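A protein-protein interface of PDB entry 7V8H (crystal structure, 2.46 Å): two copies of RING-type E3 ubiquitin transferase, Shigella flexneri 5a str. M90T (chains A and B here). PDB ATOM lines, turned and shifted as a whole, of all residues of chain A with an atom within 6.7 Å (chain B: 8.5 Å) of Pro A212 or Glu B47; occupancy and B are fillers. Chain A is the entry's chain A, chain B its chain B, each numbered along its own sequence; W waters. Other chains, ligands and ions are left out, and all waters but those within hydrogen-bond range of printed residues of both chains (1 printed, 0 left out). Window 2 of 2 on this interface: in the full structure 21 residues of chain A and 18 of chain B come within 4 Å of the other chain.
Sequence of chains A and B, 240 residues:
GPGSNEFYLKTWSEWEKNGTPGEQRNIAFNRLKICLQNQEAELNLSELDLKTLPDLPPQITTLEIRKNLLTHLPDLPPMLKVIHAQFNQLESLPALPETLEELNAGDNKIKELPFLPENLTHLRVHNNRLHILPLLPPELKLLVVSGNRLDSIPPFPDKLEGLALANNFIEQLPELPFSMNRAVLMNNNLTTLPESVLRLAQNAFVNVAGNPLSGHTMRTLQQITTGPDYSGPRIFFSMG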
ATOM      1  N   ASN A 188       5.199 -14.754 -27.841  1.00  0.00           N
ATOM      2  CA  ASN A 188       5.616 -16.143 -27.840  1.00  0.00           C
ATOM      3  C   ASN A 188       4.473 -16.989 -27.306  1.00  0.00           C
ATOM      4  O   ASN A 188       3.313 -16.578 -27.372  1.00  0.00           O
ATOM      5  CB  ASN A 188       6.894 -16.318 -27.015  1.00  0.00           C
ATOM      6  CG  ASN A 188       8.149 -16.039 -27.828  1.00  0.00           C
ATOM      7  OD1 ASN A 188       8.661 -16.929 -28.506  1.00  0.00           O
ATOM      8  ND2 ASN A 188       8.649 -14.806 -27.764  1.00  0.00           N
ATOM      9  N   ASN A 189       4.769 -18.160 -26.777  1.00  0.00           N
ATOM     10  CA  ASN A 189       3.745 -19.055 -26.257  1.00  0.00           C
ATOM     11  C   ASN A 189       3.981 -19.366 -24.778  1.00  0.00           C
ATOM     12  O   ASN A 189       3.737 -20.475 -24.309  1.00  0.00           O
ATOM     13  CB  ASN A 189       3.702 -20.338 -27.081  1.00  0.00           C
ATOM     14  CG  ASN A 189       2.290 -20.858 -27.303  1.00  0.00           C
ATOM     15  OD1 ASN A 189       1.309 -20.326 -26.759  1.00  0.00           O
ATOM     16  ND2 ASN A 189       2.183 -21.933 -28.078  1.00  0.00           N
ATOM     17  N   LEU A 190       4.453 -18.387 -24.013  1.00  0.00           N
ATOM     18  CA  LEU A 190       4.676 -18.597 -22.591  1.00  0.00           C
ATOM     19  C   LEU A 190       3.345 -18.582 -21.857  1.00  0.00           C
ATOM     20  O   LEU A 190       2.549 -17.656 -22.039  1.00  0.00           O
ATOM     21  CB  LEU A 190       5.574 -17.498 -22.012  1.00  0.00           C
ATOM     22  CG  LEU A 190       6.974 -17.266 -22.574  1.00  0.00           C
ATOM     23  CD1 LEU A 190       7.648 -16.141 -21.800  1.00  0.00           C
ATOM     24  CD2 LEU A 190       7.777 -18.549 -22.476  1.00  0.00           C
ATOM     25  N   THR A 191       3.120 -19.589 -20.997  1.00  0.00           N
ATOM     26  CA  THR A 191       2.021 -19.562 -20.030  1.00  0.00           C
ATOM     27  C   THR A 191       2.477 -19.273 -18.606  1.00  0.00           C
ATOM     28  O   THR A 191       1.636 -18.953 -17.758  1.00  0.00           O
ATOM     29  CB  THR A 191       1.266 -20.892 -20.007  1.00  0.00           C
ATOM     30  OG1 THR A 191       2.135 -21.899 -19.491  1.00  0.00           O
ATOM     31  CG2 THR A 191       0.787 -21.282 -21.399  1.00  0.00           C
ATOM     32  N   THR A 192       3.764 -19.455 -18.310  1.00  0.00           N
ATOM     33  CA  THR A 192       4.345 -19.121 -17.025  1.00  0.00           C
ATOM     34  C   THR A 192       5.681 -18.442 -17.257  1.00  0.00           C
ATOM     35  O   THR A 192       6.248 -18.494 -18.349  1.00  0.00           O
ATOM     36  CB  THR A 192       4.557 -20.357 -16.138  1.00  0.00           C
ATOM     37  OG1 THR A 192       5.650 -21.114 -16.660  1.00  0.00           O
ATOM     38  CG2 THR A 192       3.306 -21.247 -16.097  1.00  0.00           C
ATOM     39  N   VAL A 208       6.683  -9.044 -21.565  1.00  0.00           N
ATOM     40  CA  VAL A 208       6.168 -10.362 -21.918  1.00  0.00           C
ATOM     41  C   VAL A 208       4.768 -10.272 -22.511  1.00  0.00           C
ATOM     42  O   VAL A 208       4.055 -11.263 -22.552  1.00  0.00           O
ATOM     43  CB  VAL A 208       6.183 -11.313 -20.707  1.00  0.00           C
ATOM     44  CG1 VAL A 208       7.618 -11.662 -20.299  1.00  0.00           C
ATOM     45  CG2 VAL A 208       5.420 -10.690 -19.539  1.00  0.00           C
ATOM     46  N   ALA A 209       4.371  -9.079 -22.959  1.00  0.00           N
ATOM     47  CA  ALA A 209       3.091  -8.887 -23.626  1.00  0.00           C
ATOM     48  C   ALA A 209       2.923  -9.866 -24.778  1.00  0.00           C
ATOM     49  O   ALA A 209       3.888 -10.303 -25.398  1.00  0.00           O
ATOM     50  CB  ALA A 209       2.981  -7.456 -24.164  1.00  0.00           C
ATOM     51  N   GLY A 210       1.686 -10.205 -25.080  1.00  0.00           N
ATOM     52  CA  GLY A 210       1.476 -11.083 -26.204  1.00  0.00           C
ATOM     53  C   GLY A 210       1.726 -12.537 -25.911  1.00  0.00           C
ATOM     54  O   GLY A 210       1.718 -13.351 -26.838  1.00  0.00           O
ATOM     55  N   ASN A 211       1.930 -12.889 -24.669  1.00  0.00           N
ATOM     56  CA  ASN A 211       2.051 -14.263 -24.271  1.00  0.00           C
ATOM     57  C   ASN A 211       0.805 -14.675 -23.512  1.00  0.00           C
ATOM     58  O   ASN A 211       0.258 -13.864 -22.763  1.00  0.00           O
ATOM     59  CB  ASN A 211       3.278 -14.462 -23.383  1.00  0.00           C
ATOM     60  CG  ASN A 211       4.576 -14.450 -24.174  1.00  0.00           C
ATOM     61  OD1 ASN A 211       5.007 -15.480 -24.677  1.00  0.00           O
ATOM     62  ND2 ASN A 211       5.206 -13.287 -24.275  1.00  0.00           N
ATOM     63  N   PRO A 212       0.322 -15.904 -23.687  1.00  0.00           N
ATOM     64  CA  PRO A 212      -0.911 -16.346 -22.975  1.00  0.00           C
ATOM     65  C   PRO A 212      -0.645 -16.771 -21.538  1.00  0.00           C
ATOM     66  O   PRO A 212      -0.782 -17.947 -21.163  1.00  0.00           O
ATOM     67  CB  PRO A 212      -1.373 -17.532 -23.831  1.00  0.00           C
ATOM     68  CG  PRO A 212      -0.082 -18.160 -24.248  1.00  0.00           C
ATOM     69  CD  PRO A 212       0.854 -16.962 -24.568  1.00  0.00           C
ATOM     70  N   LEU A 213      -0.245 -15.825 -20.697  1.00  0.00           N
ATOM     71  CA  LEU A 213       0.051 -16.185 -19.314  1.00  0.00           C
ATOM     72  C   LEU A 213      -1.212 -16.687 -18.620  1.00  0.00           C
ATOM     73  O   LEU A 213      -2.269 -16.053 -18.695  1.00  0.00           O
ATOM     74  CB  LEU A 213       0.623 -14.988 -18.566  1.00  0.00           C
ATOM     75  CG  LEU A 213       1.937 -14.441 -19.111  1.00  0.00           C
ATOM     76  CD1 LEU A 213       2.386 -13.290 -18.227  1.00  0.00           C
ATOM     77  CD2 LEU A 213       2.997 -15.531 -19.201  1.00  0.00           C
ATOM     78  N   SER A 214      -1.085 -17.810 -17.922  1.00  0.00           N
ATOM     79  CA  SER A 214      -2.213 -18.444 -17.260  1.00  0.00           C
ATOM     80  C   SER A 214      -2.735 -17.564 -16.133  1.00  0.00           C
ATOM     81  O   SER A 214      -2.081 -16.614 -15.697  1.00  0.00           O
ATOM     82  CB  SER A 214      -1.812 -19.801 -16.686  1.00  0.00           C
ATOM     83  OG  SER A 214      -0.897 -19.640 -15.605  1.00  0.00           O
ATOM     84  N   GLY A 215      -3.936 -17.900 -15.657  1.00  0.00           N
ATOM     85  CA  GLY A 215      -4.500 -17.182 -14.527  1.00  0.00           C
ATOM     86  C   GLY A 215      -3.672 -17.313 -13.264  1.00  0.00           C
ATOM     87  O   GLY A 215      -3.454 -16.331 -12.550  1.00  0.00           O
ATOM     88  N   SER A 238       0.139  -8.152 -21.400  1.00  0.00           N
ATOM     89  CA  SER A 238      -1.130  -7.804 -22.011  1.00  0.00           C
ATOM     90  C   SER A 238      -2.136  -8.903 -21.731  1.00  0.00           C
ATOM     91  O   SER A 238      -1.785 -10.014 -21.329  1.00  0.00           O
ATOM     92  CB  SER A 238      -0.998  -7.548 -23.525  1.00  0.00           C
ATOM     93  OG  SER A 238      -0.610  -8.701 -24.238  1.00  0.00           O
ATOM     94  N   GLY B  22      -0.090 -34.630 -28.358  1.00  0.00           N
ATOM     95  CA  GLY B  22      -0.193 -33.285 -27.796  1.00  0.00           C
ATOM     96  C   GLY B  22      -1.334 -32.425 -28.317  1.00  0.00           C
ATOM     97  O   GLY B  22      -1.724 -31.468 -27.640  1.00  0.00           O
ATOM     98  N   GLU B  23      -1.859 -32.715 -29.513  1.00  0.00           N
ATOM     99  CA  GLU B  23      -2.972 -31.940 -30.054  1.00  0.00           C
ATOM    100  C   GLU B  23      -4.196 -32.067 -29.152  1.00  0.00           C
ATOM    101  O   GLU B  23      -4.617 -33.176 -28.808  1.00  0.00           O
ATOM    102  CB  GLU B  23      -3.328 -32.421 -31.465  1.00  0.00           C
ATOM    103  CG  GLU B  23      -2.157 -32.584 -32.410  1.00  0.00           C
ATOM    104  CD  GLU B  23      -2.584 -32.967 -33.822  1.00  0.00           C
ATOM    105  OE1 GLU B  23      -3.343 -32.194 -34.452  1.00  0.00           O
ATOM    106  OE2 GLU B  23      -2.154 -34.036 -34.319  1.00  0.00           O
ATOM    107  N   GLN B  24      -4.763 -30.936 -28.757  1.00  0.00           N
ATOM    108  CA  GLN B  24      -5.946 -30.933 -27.898  1.00  0.00           C
ATOM    109  C   GLN B  24      -7.230 -31.006 -28.716  1.00  0.00           C
ATOM    110  O   GLN B  24      -8.089 -30.129 -28.611  1.00  0.00           O
ATOM    111  CB  GLN B  24      -5.941 -29.696 -27.021  1.00  0.00           C
ATOM    112  CG  GLN B  24      -4.664 -29.510 -26.241  1.00  0.00           C
ATOM    113  CD  GLN B  24      -4.743 -28.281 -25.379  1.00  0.00           C
ATOM    114  OE1 GLN B  24      -5.705 -28.120 -24.623  1.00  0.00           O
ATOM    115  NE2 GLN B  24      -3.744 -27.394 -25.489  1.00  0.00           N
ATOM    116  N   ILE B  27     -10.888 -30.778 -26.826  1.00  0.00           N
ATOM    117  CA  ILE B  27     -11.425 -29.440 -26.606  1.00  0.00           C
ATOM    118  C   ILE B  27     -11.895 -28.821 -27.924  1.00  0.00           C
ATOM    119  O   ILE B  27     -12.967 -28.207 -27.988  1.00  0.00           O
ATOM    120  CB  ILE B  27     -10.386 -28.554 -25.894  1.00  0.00           C
ATOM    121  CG1 ILE B  27     -10.090 -29.094 -24.477  1.00  0.00           C
ATOM    122  CG2 ILE B  27     -10.821 -27.093 -25.915  1.00  0.00           C
ATOM    123  CD1 ILE B  27      -8.949 -28.430 -23.798  1.00  0.00           C
ATOM    124  N   ARG B  31     -15.588 -27.254 -28.953  1.00  0.00           N
ATOM    125  CA  ARG B  31     -15.800 -25.905 -29.469  1.00  0.00           C
ATOM    126  C   ARG B  31     -16.445 -25.952 -30.855  1.00  0.00           C
ATOM    127  O   ARG B  31     -17.289 -25.110 -31.189  1.00  0.00           O
ATOM    128  CB  ARG B  31     -14.474 -25.141 -29.498  1.00  0.00           C
ATOM    129  CG  ARG B  31     -13.831 -24.944 -28.121  1.00  0.00           C
ATOM    130  CD  ARG B  31     -13.309 -23.519 -27.938  1.00  0.00           C
ATOM    131  NE  ARG B  31     -12.507 -23.387 -26.721  1.00  0.00           N
ATOM    132  CZ  ARG B  31     -11.236 -22.985 -26.674  1.00  0.00           C
ATOM    133  NH1 ARG B  31     -10.567 -22.655 -27.783  1.00  0.00           N
ATOM    134  NH2 ARG B  31     -10.626 -22.910 -25.502  1.00  0.00           N
ATOM    135  N   ASN B  44     -13.267 -20.267 -32.244  1.00  0.00           N
ATOM    136  CA  ASN B  44     -11.963 -19.984 -31.629  1.00  0.00           C
ATOM    137  C   ASN B  44     -11.218 -21.289 -31.296  1.00  0.00           C
ATOM    138  O   ASN B  44     -11.468 -21.919 -30.262  1.00  0.00           O
ATOM    139  CB  ASN B  44     -12.162 -19.112 -30.393  1.00  0.00           C
ATOM    140  CG  ASN B  44     -10.854 -18.757 -29.691  1.00  0.00           C
ATOM    141  OD1 ASN B  44      -9.764 -19.192 -30.074  1.00  0.00           O
ATOM    142  ND2 ASN B  44     -10.960 -17.912 -28.686  1.00  0.00           N
ATOM    143  N   LEU B  45     -10.269 -21.679 -32.150  1.00  0.00           N
ATOM    144  CA  LEU B  45      -9.431 -22.858 -31.926  1.00  0.00           C
ATOM    145  C   LEU B  45      -7.976 -22.481 -31.680  1.00  0.00           C
ATOM    146  O   LEU B  45      -7.061 -23.275 -31.908  1.00  0.00           O
ATOM    147  CB  LEU B  45      -9.525 -23.825 -33.099  1.00  0.00           C
ATOM    148  CG  LEU B  45     -10.950 -24.307 -33.393  1.00  0.00           C
ATOM    149  CD1 LEU B  45     -10.966 -25.208 -34.613  1.00  0.00           C
ATOM    150  CD2 LEU B  45     -11.537 -25.050 -32.197  1.00  0.00           C
ATOM    151  N   SER B  46      -7.752 -21.266 -31.217  1.00  0.00           N
ATOM    152  CA  SER B  46      -6.400 -20.821 -30.972  1.00  0.00           C
ATOM    153  C   SER B  46      -5.813 -21.536 -29.758  1.00  0.00           C
ATOM    154  O   SER B  46      -6.535 -21.971 -28.858  1.00  0.00           O
ATOM    155  CB  SER B  46      -6.387 -19.315 -30.748  1.00  0.00           C
ATOM    156  OG  SER B  46      -7.207 -18.994 -29.651  1.00  0.00           O
ATOM    157  N   GLU B  47      -4.487 -21.704 -29.781  1.00  0.00           N
ATOM    158  CA  GLU B  47      -3.718 -22.186 -28.636  1.00  0.00           C
ATOM    159  C   GLU B  47      -4.106 -23.606 -28.217  1.00  0.00           C
ATOM    160  O   GLU B  47      -4.163 -23.913 -27.032  1.00  0.00           O
ATOM    161  CB  GLU B  47      -3.848 -21.213 -27.456  1.00  0.00           C
ATOM    162  CG  GLU B  47      -3.150 -19.868 -27.663  1.00  0.00           C
ATOM    163  CD  GLU B  47      -3.754 -18.718 -26.854  1.00  0.00           C
ATOM    164  OE1 GLU B  47      -4.203 -18.939 -25.700  1.00  0.00           O
ATOM    165  OE2 GLU B  47      -3.768 -17.572 -27.369  1.00  0.00           O
ATOM    166  N   LEU B  48      -4.374 -24.483 -29.185  1.00  0.00           N
ATOM    167  CA  LEU B  48      -4.716 -25.877 -28.901  1.00  0.00           C
ATOM    168  C   LEU B  48      -3.698 -26.871 -29.475  1.00  0.00           C
ATOM    169  O   LEU B  48      -4.010 -28.062 -29.586  1.00  0.00           O
ATOM    170  CB  LEU B  48      -6.123 -26.207 -29.421  1.00  0.00           C
ATOM    171  CG  LEU B  48      -7.334 -25.440 -28.850  1.00  0.00           C
ATOM    172  CD1 LEU B  48      -8.622 -25.869 -29.535  1.00  0.00           C
ATOM    173  CD2 LEU B  48      -7.477 -25.579 -27.329  1.00  0.00           C
ATOM    174  N   ASP B  49      -2.497 -26.407 -29.863  1.00  0.00           N
ATOM    175  CA  ASP B  49      -1.443 -27.254 -30.447  1.00  0.00           C
ATOM    176  C   ASP B  49      -1.930 -28.046 -31.662  1.00  0.00           C
ATOM    177  O   ASP B  49      -1.519 -29.192 -31.864  1.00  0.00           O
ATOM    178  CB  ASP B  49      -0.851 -28.246 -29.434  1.00  0.00           C
ATOM    179  CG  ASP B  49      -0.504 -27.614 -28.110  1.00  0.00           C
ATOM    180  OD1 ASP B  49       0.691 -27.267 -27.938  1.00  0.00           O
ATOM    181  OD2 ASP B  49      -1.399 -27.544 -27.219  1.00  0.00           O
ATOM    182  N   LEU B  50      -2.812 -27.469 -32.479  1.00  0.00           N
ATOM    183  CA  LEU B  50      -3.459 -28.242 -33.537  1.00  0.00           C
ATOM    184  C   LEU B  50      -2.596 -28.336 -34.788  1.00  0.00           C
ATOM    185  O   LEU B  50      -2.136 -27.323 -35.326  1.00  0.00           O
ATOM    186  CB  LEU B  50      -4.823 -27.646 -33.900  1.00  0.00           C
ATOM    187  CG  LEU B  50      -5.866 -27.493 -32.797  1.00  0.00           C
ATOM    188  CD1 LEU B  50      -7.215 -27.070 -33.378  1.00  0.00           C
ATOM    189  CD2 LEU B  50      -6.000 -28.777 -31.949  1.00  0.00           C
ATOM    190  N   GLU B  64     -10.753 -17.767 -35.551  1.00  0.00           N
ATOM    191  CA  GLU B  64      -9.662 -17.425 -34.639  1.00  0.00           C
ATOM    192  C   GLU B  64      -8.889 -18.700 -34.353  1.00  0.00           C
ATOM    193  O   GLU B  64      -9.394 -19.594 -33.671  1.00  0.00           O
ATOM    194  CB  GLU B  64     -10.244 -16.778 -33.382  1.00  0.00           C
ATOM    195  CG  GLU B  64      -9.324 -16.483 -32.245  1.00  0.00           C
ATOM    196  CD  GLU B  64      -8.319 -15.401 -32.586  1.00  0.00           C
ATOM    197  OE1 GLU B  64      -8.636 -14.186 -32.423  1.00  0.00           O
ATOM    198  OE2 GLU B  64      -7.173 -15.781 -32.922  1.00  0.00           O
ATOM    199  N   ILE B  65      -7.691 -18.806 -34.923  1.00  0.00           N
ATOM    200  CA  ILE B  65      -6.900 -20.033 -34.881  1.00  0.00           C
ATOM    201  C   ILE B  65      -5.413 -19.727 -34.709  1.00  0.00           C
ATOM    202  O   ILE B  65      -4.558 -20.545 -35.061  1.00  0.00           O
ATOM    203  CB  ILE B  65      -7.110 -20.881 -36.153  1.00  0.00           C
ATOM    204  CG1 ILE B  65      -6.795 -20.073 -37.398  1.00  0.00           C
ATOM    205  CG2 ILE B  65      -8.524 -21.417 -36.233  1.00  0.00           C
ATOM    206  CD1 ILE B  65      -6.947 -20.846 -38.671  1.00  0.00           C
ATOM    207  N   ARG B  66      -5.088 -18.563 -34.162  1.00  0.00           N
ATOM    208  CA  ARG B  66      -3.690 -18.222 -33.989  1.00  0.00           C
ATOM    209  C   ARG B  66      -2.996 -19.218 -33.047  1.00  0.00           C
ATOM    210  O   ARG B  66      -3.626 -19.874 -32.219  1.00  0.00           O
ATOM    211  CB  ARG B  66      -3.561 -16.789 -33.454  1.00  0.00           C
ATOM    212  CG  ARG B  66      -4.026 -16.689 -32.024  1.00  0.00           C
ATOM    213  CD  ARG B  66      -3.821 -15.341 -31.392  1.00  0.00           C
ATOM    214  NE  ARG B  66      -4.987 -14.507 -31.588  1.00  0.00           N
ATOM    215  CZ  ARG B  66      -4.955 -13.185 -31.629  1.00  0.00           C
ATOM    216  NH1 ARG B  66      -3.799 -12.551 -31.469  1.00  0.00           N
ATOM    217  NH2 ARG B  66      -6.081 -12.514 -31.825  1.00  0.00           N
ATOM    218  N   LYS B  67      -1.676 -19.335 -33.192  1.00  0.00           N
ATOM    219  CA  LYS B  67      -0.833 -20.064 -32.236  1.00  0.00           C
ATOM    220  C   LYS B  67      -1.167 -21.558 -32.183  1.00  0.00           C
ATOM    221  O   LYS B  67      -1.422 -22.133 -31.124  1.00  0.00           O
ATOM    222  CB  LYS B  67      -0.907 -19.423 -30.847  1.00  0.00           C
ATOM    223  CG  LYS B  67      -0.150 -18.080 -30.812  1.00  0.00           C
ATOM    224  CD  LYS B  67       0.282 -17.706 -29.436  1.00  0.00           C
ATOM    225  CE  LYS B  67       0.548 -16.215 -29.326  1.00  0.00           C
ATOM    226  NZ  LYS B  67       1.914 -15.773 -29.654  1.00  0.00           N
ATOM    227  N   ASN B  68      -1.180 -22.191 -33.353  1.00  0.00           N
ATOM    228  CA  ASN B  68      -1.297 -23.638 -33.404  1.00  0.00           C
ATOM    229  C   ASN B  68      -0.110 -24.141 -34.196  1.00  0.00           C
ATOM    230  O   ASN B  68       0.914 -23.458 -34.291  1.00  0.00           O
ATOM    231  CB  ASN B  68      -2.625 -24.065 -34.042  1.00  0.00           C
ATOM    232  CG  ASN B  68      -3.775 -24.035 -33.054  1.00  0.00           C
ATOM    233  OD1 ASN B  68      -3.857 -24.878 -32.151  1.00  0.00           O
ATOM    234  ND2 ASN B  68      -4.662 -23.042 -33.201  1.00  0.00           N
ATOM    235  N   LEU B  69      -0.241 -25.310 -34.801  1.00  0.00           N
ATOM    236  CA  LEU B  69       0.841 -25.881 -35.588  1.00  0.00           C
ATOM    237  C   LEU B  69       0.335 -26.217 -36.987  1.00  0.00           C
ATOM    238  O   LEU B  69       0.773 -27.188 -37.608  1.00  0.00           O
ATOM    239  CB  LEU B  69       1.406 -27.119 -34.898  1.00  0.00           C
ATOM    240  CG  LEU B  69       2.478 -26.943 -33.810  1.00  0.00           C
ATOM    241  CD1 LEU B  69       3.816 -26.490 -34.365  1.00  0.00           C
ATOM    242  CD2 LEU B  69       2.053 -26.005 -32.718  1.00  0.00           C
ATOM    243  N   GLN B  86      -2.266 -16.099 -37.401  1.00  0.00           N
ATOM    244  CA  GLN B  86      -0.861 -15.829 -37.145  1.00  0.00           C
ATOM    245  C   GLN B  86      -0.273 -16.876 -36.187  1.00  0.00           C
ATOM    246  O   GLN B  86      -0.985 -17.523 -35.419  1.00  0.00           O
ATOM    247  CB  GLN B  86      -0.680 -14.409 -36.578  1.00  0.00           C
ATOM    248  CG  GLN B  86      -1.318 -14.160 -35.230  1.00  0.00           C
ATOM    249  CD  GLN B  86      -2.742 -13.622 -35.337  1.00  0.00           C
ATOM    250  OE1 GLN B  86      -3.516 -14.065 -36.194  1.00  0.00           O
ATOM    251  NE2 GLN B  86      -3.107 -12.685 -34.444  1.00  0.00           N
ATOM    252  N   PHE B  87       1.053 -17.051 -36.264  1.00  0.00           N
ATOM    253  CA  PHE B  87       1.807 -18.031 -35.474  1.00  0.00           C
ATOM    254  C   PHE B  87       1.312 -19.459 -35.741  1.00  0.00           C
ATOM    255  O   PHE B  87       0.777 -20.136 -34.871  1.00  0.00           O
ATOM    256  CB  PHE B  87       1.769 -17.683 -33.972  1.00  0.00           C
ATOM    257  CG  PHE B  87       2.442 -16.395 -33.652  1.00  0.00           C
ATOM    258  CD1 PHE B  87       3.812 -16.332 -33.512  1.00  0.00           C
ATOM    259  CD2 PHE B  87       1.715 -15.228 -33.552  1.00  0.00           C
ATOM    260  CE1 PHE B  87       4.445 -15.120 -33.243  1.00  0.00           C
ATOM    261  CE2 PHE B  87       2.336 -14.017 -33.290  1.00  0.00           C
ATOM    262  CZ  PHE B  87       3.704 -13.961 -33.136  1.00  0.00           C
ATOM    263  N   ASN B  88       1.499 -19.902 -36.978  1.00  0.00           N
ATOM    264  CA  ASN B  88       1.280 -21.294 -37.354  1.00  0.00           C
ATOM    265  C   ASN B  88       2.514 -21.710 -38.153  1.00  0.00           C
ATOM    266  O   ASN B  88       3.585 -21.104 -38.047  1.00  0.00           O
ATOM    267  CB  ASN B  88      -0.041 -21.470 -38.129  1.00  0.00           C
ATOM    268  CG  ASN B  88      -1.235 -21.589 -37.219  1.00  0.00           C
ATOM    269  OD1 ASN B  88      -1.493 -22.659 -36.670  1.00  0.00           O
ATOM    270  ND2 ASN B  88      -1.956 -20.478 -37.013  1.00  0.00           N
HETATM  271  O   HOH W   1       0.897 -12.505 -29.958  1.00  0.00           O
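Of the 14 printed residues of chain A, 4 touch a printed residue of chain B. Printed residues of chain A that touch a printed residue of chain B: Asn A188, Asn A189, Gly A210 and Pro A212. Of the 21 printed residues of chain B, 2 touch a printed residue of chain A. Among the printed residues, no Asp or Glu carboxylate lies within 4 Å of a Lys or Arg side-chain nitrogen of the other chain.
OD1 of Asn A189 touches CD of Lys B67, 3.9 Å away. Gly A210 touches Lys B67 (O to NZ, 3.7 Å). OE1 of Glu B47 touches CB of Pro A212, 3.7 Å away.
No position is printed for both chains. Of the 4 pairs that touch across the chains among the printed residues, none has its exchanged pair printed and touching as well.
Water W1 bridges the backbone carbonyl oxygen of Gly A210 (3.3 Å) and the side-chain amino group of Lys B67 (3.4 Å).
The side-chain amino group (NZ) of Lys B67 lies within hydrogen-bond range of the backbone carbonyl oxygen (O) of Asn A188 (2.8 Å).
N of Asn A188 sits close to OD1 of Asn A211 (3.3 Å). The side-chain amide oxygen of Asn A211 lies within hydrogen-bond range of the backbone NH of Asn A189, at 3.4 Å. The backbone NH (N) of Gly A210 lies within hydrogen-bond range of the side-chain hydroxyl (OG) of Ser A238 (2.9 Å). N of Glu B47 is in hydrogen-bond range of O of Lys B67 (3.4 Å). The backbone NH (N) of Lys B67 is in hydrogen-bond range of the backbone carbonyl oxygen (O) of Gln B86 (3.0 Å). O of Phe B87 is in hydrogen-bond range of N of Lys B67 (3.1 Å).
Of the printed residues of chain B, Asn A188 touches Lys B67. Printed residues of chain B within 4 Å of Asn A189: Lys B67 (3.9 Å). Printed residues of chain B within 4 Å of Gly A210: Lys B67. Pro A212 touches just one residue of chain B: Glu B47. Ser A238 touches none of the printed residues of chain B. Glu B47 touches just one residue of chain A: Pro A212 (3.7 Å). Asp B49 touches none of the printed residues of chain A. Of the printed residues of chain A, Lys B67 touches Asn A188, Asn A189 and Gly A210. The nearest printed residue of chain B that does not touch Gly A210 is Phe B87 (6.5 Å).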
